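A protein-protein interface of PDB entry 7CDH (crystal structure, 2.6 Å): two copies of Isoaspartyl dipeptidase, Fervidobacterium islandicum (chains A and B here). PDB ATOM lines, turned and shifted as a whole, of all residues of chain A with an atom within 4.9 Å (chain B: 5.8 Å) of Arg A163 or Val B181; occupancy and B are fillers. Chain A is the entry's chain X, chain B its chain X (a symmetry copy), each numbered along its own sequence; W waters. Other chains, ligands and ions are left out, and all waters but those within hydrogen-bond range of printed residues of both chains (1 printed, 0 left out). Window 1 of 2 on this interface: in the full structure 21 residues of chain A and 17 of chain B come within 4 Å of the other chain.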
ATOM      1  N   GLU A  70      12.788   4.924 -19.825  1.00  0.00           N
ATOM      2  CA  GLU A  70      11.897   4.366 -20.884  1.00  0.00           C
ATOM      3  C   GLU A  70      12.056   2.840 -20.982  1.00  0.00           C
ATOM      4  O   GLU A  70      11.138   2.208 -21.510  1.00  0.00           O
ATOM      5  CB  GLU A  70      12.206   4.948 -22.269  1.00  0.00           C
ATOM      6  CG  GLU A  70      11.773   6.386 -22.438  1.00  0.00           C
ATOM      7  CD  GLU A  70      12.884   7.413 -22.273  1.00  0.00           C
ATOM      8  OE1 GLU A  70      12.726   8.543 -22.805  1.00  0.00           O
ATOM      9  OE2 GLU A  70      13.908   7.077 -21.619  1.00  0.00           O
ATOM     10  N   THR A  99      10.393  12.033 -19.989  1.00  0.00           N
ATOM     11  CA  THR A  99       9.335  10.995 -19.924  1.00  0.00           C
ATOM     12  C   THR A  99       8.870  10.787 -18.488  1.00  0.00           C
ATOM     13  O   THR A  99       7.668  10.759 -18.287  1.00  0.00           O
ATOM     14  CB  THR A  99       9.832   9.685 -20.516  1.00  0.00           C
ATOM     15  OG1 THR A  99      10.463  10.074 -21.735  1.00  0.00           O
ATOM     16  CG2 THR A  99       8.697   8.724 -20.757  1.00  0.00           C
ATOM     17  N   TYR A 130       7.071  15.784 -19.743  1.00  0.00           N
ATOM     18  CA  TYR A 130       6.413  15.295 -20.973  1.00  0.00           C
ATOM     19  C   TYR A 130       4.901  15.375 -20.808  1.00  0.00           C
ATOM     20  O   TYR A 130       4.221  15.794 -21.729  1.00  0.00           O
ATOM     21  CB  TYR A 130       6.745  13.839 -21.283  1.00  0.00           C
ATOM     22  CG  TYR A 130       7.924  13.573 -22.185  1.00  0.00           C
ATOM     23  CD1 TYR A 130       9.060  14.374 -22.208  1.00  0.00           C
ATOM     24  CD2 TYR A 130       7.918  12.438 -22.991  1.00  0.00           C
ATOM     25  CE1 TYR A 130      10.149  14.072 -23.018  1.00  0.00           C
ATOM     26  CE2 TYR A 130       8.982  12.141 -23.830  1.00  0.00           C
ATOM     27  CZ  TYR A 130      10.107  12.948 -23.832  1.00  0.00           C
ATOM     28  OH  TYR A 130      11.149  12.582 -24.649  1.00  0.00           O
ATOM     29  N   ALA A 158       5.442  16.666 -24.519  1.00  0.00           N
ATOM     30  CA  ALA A 158       5.528  15.744 -25.661  1.00  0.00           C
ATOM     31  C   ALA A 158       4.281  15.912 -26.517  1.00  0.00           C
ATOM     32  O   ALA A 158       3.167  15.886 -25.976  1.00  0.00           O
ATOM     33  CB  ALA A 158       5.690  14.315 -25.205  1.00  0.00           C
ATOM     34  N   ASP A 161       4.210  11.848 -30.387  1.00  0.00           N
ATOM     35  CA  ASP A 161       5.183  10.910 -29.763  1.00  0.00           C
ATOM     36  C   ASP A 161       4.429   9.811 -29.008  1.00  0.00           C
ATOM     37  O   ASP A 161       3.408  10.108 -28.382  1.00  0.00           O
ATOM     38  CB  ASP A 161       6.124  11.616 -28.785  1.00  0.00           C
ATOM     39  CG  ASP A 161       7.328  10.779 -28.420  1.00  0.00           C
ATOM     40  OD1 ASP A 161       7.222   9.962 -27.475  1.00  0.00           O
ATOM     41  OD2 ASP A 161       8.344  10.915 -29.123  1.00  0.00           O
ATOM     42  N   HIS A 162       4.962   8.597 -29.038  1.00  0.00           N
ATOM     43  CA  HIS A 162       4.368   7.408 -28.394  1.00  0.00           C
ATOM     44  C   HIS A 162       4.469   7.515 -26.852  1.00  0.00           C
ATOM     45  O   HIS A 162       3.726   6.809 -26.204  1.00  0.00           O
ATOM     46  CB  HIS A 162       4.974   6.139 -29.013  1.00  0.00           C
ATOM     47  CG  HIS A 162       6.423   5.937 -28.729  1.00  0.00           C
ATOM     48  ND1 HIS A 162       7.411   6.361 -29.586  1.00  0.00           N
ATOM     49  CD2 HIS A 162       7.060   5.339 -27.713  1.00  0.00           C
ATOM     50  CE1 HIS A 162       8.592   6.027 -29.110  1.00  0.00           C
ATOM     51  NE2 HIS A 162       8.395   5.412 -27.970  1.00  0.00           N
ATOM     52  N   ARG A 163       5.283   8.409 -26.291  1.00  0.00           N
ATOM     53  CA  ARG A 163       5.407   8.642 -24.826  1.00  0.00           C
ATOM     54  C   ARG A 163       4.591   9.865 -24.370  1.00  0.00           C
ATOM     55  O   ARG A 163       4.632  10.221 -23.142  1.00  0.00           O
ATOM     56  CB  ARG A 163       6.872   8.809 -24.431  1.00  0.00           C
ATOM     57  CG  ARG A 163       7.740   7.581 -24.691  1.00  0.00           C
ATOM     58  CD  ARG A 163       9.193   8.011 -24.834  1.00  0.00           C
ATOM     59  NE  ARG A 163       9.412   8.626 -26.143  1.00  0.00           N
ATOM     60  CZ  ARG A 163      10.569   9.114 -26.590  1.00  0.00           C
ATOM     61  NH1 ARG A 163      11.651   9.095 -25.830  1.00  0.00           N
ATOM     62  NH2 ARG A 163      10.629   9.622 -27.809  1.00  0.00           N
ATOM     63  N   SER A 164       3.834  10.485 -25.276  1.00  0.00           N
ATOM     64  CA  SER A 164       3.013  11.671 -24.942  1.00  0.00           C
ATOM     65  C   SER A 164       1.826  11.219 -24.078  1.00  0.00           C
ATOM     66  O   SER A 164       1.560  10.008 -23.986  1.00  0.00           O
ATOM     67  CB  SER A 164       2.565  12.386 -26.180  1.00  0.00           C
ATOM     68  OG  SER A 164       1.380  11.808 -26.677  1.00  0.00           O
ATOM     69  N   SER A 165       1.118  12.143 -23.459  1.00  0.00           N
ATOM     70  CA  SER A 165      -0.125  11.796 -22.747  1.00  0.00           C
ATOM     71  C   SER A 165      -1.295  12.075 -23.682  1.00  0.00           C
ATOM     72  O   SER A 165      -2.402  12.200 -23.207  1.00  0.00           O
ATOM     73  CB  SER A 165      -0.215  12.544 -21.487  1.00  0.00           C
ATOM     74  OG  SER A 165      -0.410  13.925 -21.724  1.00  0.00           O
ATOM     75  N   HIS A 195       8.682  18.706 -26.851  1.00  0.00           N
ATOM     76  CA  HIS A 195       9.302  17.478 -27.380  1.00  0.00           C
ATOM     77  C   HIS A 195       8.478  17.022 -28.578  1.00  0.00           C
ATOM     78  O   HIS A 195       7.302  16.658 -28.397  1.00  0.00           O
ATOM     79  CB  HIS A 195       9.392  16.396 -26.320  1.00  0.00           C
ATOM     80  CG  HIS A 195       9.729  15.067 -26.890  1.00  0.00           C
ATOM     81  ND1 HIS A 195      11.018  14.586 -26.887  1.00  0.00           N
ATOM     82  CD2 HIS A 195       8.959  14.157 -27.533  1.00  0.00           C
ATOM     83  CE1 HIS A 195      11.017  13.399 -27.480  1.00  0.00           C
ATOM     84  NE2 HIS A 195       9.759  13.100 -27.883  1.00  0.00           N
ATOM     85  N   MET B 142      -0.885   5.889 -13.380  1.00  0.00           N
ATOM     86  CA  MET B 142       0.547   5.843 -13.724  1.00  0.00           C
ATOM     87  C   MET B 142       1.342   5.596 -12.443  1.00  0.00           C
ATOM     88  O   MET B 142       2.266   4.782 -12.490  1.00  0.00           O
ATOM     89  CB  MET B 142       1.003   7.119 -14.406  1.00  0.00           C
ATOM     90  CG  MET B 142       2.421   7.024 -14.860  1.00  0.00           C
ATOM     91  SD  MET B 142       3.058   8.548 -15.588  1.00  0.00           S
ATOM     92  CE  MET B 142       2.182   8.589 -17.149  1.00  0.00           C
ATOM     93  N   VAL B 146       3.670   2.198 -11.369  1.00  0.00           N
ATOM     94  CA  VAL B 146       5.115   2.406 -11.062  1.00  0.00           C
ATOM     95  C   VAL B 146       5.364   1.891  -9.636  1.00  0.00           C
ATOM     96  O   VAL B 146       6.288   1.084  -9.482  1.00  0.00           O
ATOM     97  CB  VAL B 146       5.543   3.862 -11.340  1.00  0.00           C
ATOM     98  CG1 VAL B 146       6.945   4.202 -10.858  1.00  0.00           C
ATOM     99  CG2 VAL B 146       5.446   4.182 -12.812  1.00  0.00           C
ATOM    100  N   VAL B 176      -4.884   5.221 -21.690  1.00  0.00           N
ATOM    101  CA  VAL B 176      -3.962   4.310 -22.420  1.00  0.00           C
ATOM    102  C   VAL B 176      -2.554   4.916 -22.389  1.00  0.00           C
ATOM    103  O   VAL B 176      -1.615   4.172 -22.122  1.00  0.00           O
ATOM    104  CB  VAL B 176      -4.432   4.027 -23.852  1.00  0.00           C
ATOM    105  CG1 VAL B 176      -3.395   3.240 -24.622  1.00  0.00           C
ATOM    106  CG2 VAL B 176      -5.756   3.295 -23.870  1.00  0.00           C
ATOM    107  N   ALA B 177      -2.396   6.208 -22.663  1.00  0.00           N
ATOM    108  CA  ALA B 177      -1.054   6.848 -22.644  1.00  0.00           C
ATOM    109  C   ALA B 177      -0.432   6.770 -21.246  1.00  0.00           C
ATOM    110  O   ALA B 177       0.776   6.540 -21.149  1.00  0.00           O
ATOM    111  CB  ALA B 177      -1.113   8.270 -23.130  1.00  0.00           C
ATOM    112  N   ASP B 178      -1.225   6.919 -20.193  1.00  0.00           N
ATOM    113  CA  ASP B 178      -0.708   6.890 -18.799  1.00  0.00           C
ATOM    114  C   ASP B 178      -0.241   5.466 -18.468  1.00  0.00           C
ATOM    115  O   ASP B 178       0.848   5.307 -17.925  1.00  0.00           O
ATOM    116  CB  ASP B 178      -1.731   7.477 -17.829  1.00  0.00           C
ATOM    117  CG  ASP B 178      -1.829   9.007 -17.904  1.00  0.00           C
ATOM    118  OD1 ASP B 178      -1.073   9.620 -18.741  1.00  0.00           O
ATOM    119  OD2 ASP B 178      -2.678   9.603 -17.133  1.00  0.00           O
ATOM    120  N   ILE B 179      -0.970   4.439 -18.855  1.00  0.00           N
ATOM    121  CA  ILE B 179      -0.581   3.069 -18.459  1.00  0.00           C
ATOM    122  C   ILE B 179       0.593   2.621 -19.344  1.00  0.00           C
ATOM    123  O   ILE B 179       1.521   1.995 -18.819  1.00  0.00           O
ATOM    124  CB  ILE B 179      -1.810   2.142 -18.456  1.00  0.00           C
ATOM    125  CG1 ILE B 179      -1.731   1.103 -17.330  1.00  0.00           C
ATOM    126  CG2 ILE B 179      -2.015   1.486 -19.805  1.00  0.00           C
ATOM    127  CD1 ILE B 179      -1.731   1.698 -15.931  1.00  0.00           C
ATOM    128  N   ARG B 180       0.649   3.050 -20.599  1.00  0.00           N
ATOM    129  CA  ARG B 180       1.818   2.793 -21.470  1.00  0.00           C
ATOM    130  C   ARG B 180       3.057   3.443 -20.864  1.00  0.00           C
ATOM    131  O   ARG B 180       4.108   2.772 -20.743  1.00  0.00           O
ATOM    132  CB  ARG B 180       1.594   3.264 -22.904  1.00  0.00           C
ATOM    133  CG  ARG B 180       2.879   3.398 -23.698  1.00  0.00           C
ATOM    134  CD  ARG B 180       2.587   3.395 -25.175  1.00  0.00           C
ATOM    135  NE  ARG B 180       3.800   3.544 -25.974  1.00  0.00           N
ATOM    136  CZ  ARG B 180       4.779   2.636 -26.088  1.00  0.00           C
ATOM    137  NH1 ARG B 180       4.735   1.489 -25.434  1.00  0.00           N
ATOM    138  NH2 ARG B 180       5.822   2.878 -26.861  1.00  0.00           N
ATOM    139  N   VAL B 181       2.986   4.704 -20.472  1.00  0.00           N
ATOM    140  CA  VAL B 181       4.226   5.361 -19.959  1.00  0.00           C
ATOM    141  C   VAL B 181       4.605   4.764 -18.599  1.00  0.00           C
ATOM    142  O   VAL B 181       5.833   4.518 -18.351  1.00  0.00           O
ATOM    143  CB  VAL B 181       4.075   6.882 -19.947  1.00  0.00           C
ATOM    144  CG1 VAL B 181       5.099   7.546 -19.042  1.00  0.00           C
ATOM    145  CG2 VAL B 181       4.190   7.395 -21.375  1.00  0.00           C
ATOM    146  N   GLY B 182       3.603   4.515 -17.756  1.00  0.00           N
ATOM    147  CA  GLY B 182       3.844   3.903 -16.447  1.00  0.00           C
ATOM    148  C   GLY B 182       4.489   2.538 -16.604  1.00  0.00           C
ATOM    149  O   GLY B 182       5.374   2.207 -15.804  1.00  0.00           O
ATOM    150  N   GLY B 183       4.036   1.775 -17.603  1.00  0.00           N
ATOM    151  CA  GLY B 183       4.638   0.496 -18.019  1.00  0.00           C
ATOM    152  C   GLY B 183       6.113   0.630 -18.359  1.00  0.00           C
ATOM    153  O   GLY B 183       6.913  -0.211 -17.885  1.00  0.00           O
ATOM    154  N   MET B 184       6.477   1.639 -19.145  1.00  0.00           N
ATOM    155  CA  MET B 184       7.875   1.832 -19.601  1.00  0.00           C
ATOM    156  C   MET B 184       8.776   2.142 -18.387  1.00  0.00           C
ATOM    157  O   MET B 184       9.876   1.590 -18.301  1.00  0.00           O
ATOM    158  CB  MET B 184       7.968   2.968 -20.627  1.00  0.00           C
ATOM    159  CG  MET B 184       7.186   2.699 -21.901  1.00  0.00           C
ATOM    160  SD  MET B 184       7.139   4.072 -23.079  1.00  0.00           S
ATOM    161  CE  MET B 184       8.866   4.153 -23.546  1.00  0.00           C
ATOM    162  N   ILE B 185       8.344   3.017 -17.488  1.00  0.00           N
ATOM    163  CA  ILE B 185       9.148   3.436 -16.312  1.00  0.00           C
ATOM    164  C   ILE B 185       9.392   2.214 -15.414  1.00  0.00           C
ATOM    165  O   ILE B 185      10.481   2.092 -14.814  1.00  0.00           O
ATOM    166  CB  ILE B 185       8.401   4.576 -15.588  1.00  0.00           C
ATOM    167  CG1 ILE B 185       8.334   5.839 -16.454  1.00  0.00           C
ATOM    168  CG2 ILE B 185       9.004   4.879 -14.219  1.00  0.00           C
ATOM    169  CD1 ILE B 185       7.359   6.913 -15.931  1.00  0.00           C
ATOM    170  N   SER B 186       8.402   1.342 -15.297  1.00  0.00           N
ATOM    171  CA  SER B 186       8.350   0.260 -14.292  1.00  0.00           C
ATOM    172  C   SER B 186       8.840  -1.073 -14.895  1.00  0.00           C
ATOM    173  O   SER B 186       8.956  -2.077 -14.159  1.00  0.00           O
ATOM    174  CB  SER B 186       6.943   0.163 -13.741  1.00  0.00           C
ATOM    175  OG  SER B 186       6.056  -0.387 -14.692  1.00  0.00           O
HETATM  176  O   HOH W   1      10.061  -0.672 -20.000  1.00  0.00           O
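Water W1 bridges the backbone carbonyl oxygen of Met B184 (2.8 Å) and the backbone carbonyl oxygen of Glu A70 (3.4 Å).
Glu A70 touches Met B184 (O to CB, 3.4 Å).
Arg A163 touches Val B181 (O to CG2, 3.4 Å).
Arg A163 touches Met B184.
Ser A164 touches Ala B177 (O to CB, 3.3 Å).
Ala B177 touches Ser A165.
Of the printed residues of chain B, Glu A70 touches Met B184.
Arg A163 touches just these residues of chain B: Val B181 and Met B184.
Printed residues of chain B within 4 Å of Ser A165: Ala B177 (3.7 Å).
Val B181 touches one residue of chain A.
Printed residues of chain A within 4 Å of Met B184: Glu A70 and Arg A163.
The nearest residue of chain A that does not touch Val B181 is Thr A99 (4.2 Å).
The nearest printed residue of chain B that does not touch Ser A164 is Val B181 (4.5 Å).
The backbone carbonyl oxygen (O) of His A162 lies within hydrogen-bond range of the guanidinium group (NE) of Arg B180 (3.3 Å).
No position is printed for both chains.
Of the 6 pairs that touch across the chains among the printed residues, none has its exchanged pair printed and touching as well.
OE1 of Glu A70 is in hydrogen-bond range of OG1 of Thr A99, 2.9 Å away.
The side-chain carboxylate of Asp A161 is in salt-bridge range of the guanidinium group of Arg A163, 2.9 Å away.
The guanidinium group (NH1) of Arg A163 is in salt-bridge range of the side-chain carboxylate (OE1) of Glu A70 (3.3 Å).
O of Asp A161 lies within hydrogen-bond range of OG of Ser A164 (3.1 Å).
Printed residues of chain B that touch a printed residue of chain A: Ala B177, Arg B180, Val B181 and Met B184.
Hydrophobic or aromatic side chains of chain B within 4 Å of the printed part of chain A: Ala B177, Val B181 and Met B184.
Along chain B the printed residues that touch a printed residue of chain A span positions 177 to 184.
Of the 10 printed residues of chain A, 5 touch a printed residue of chain B.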
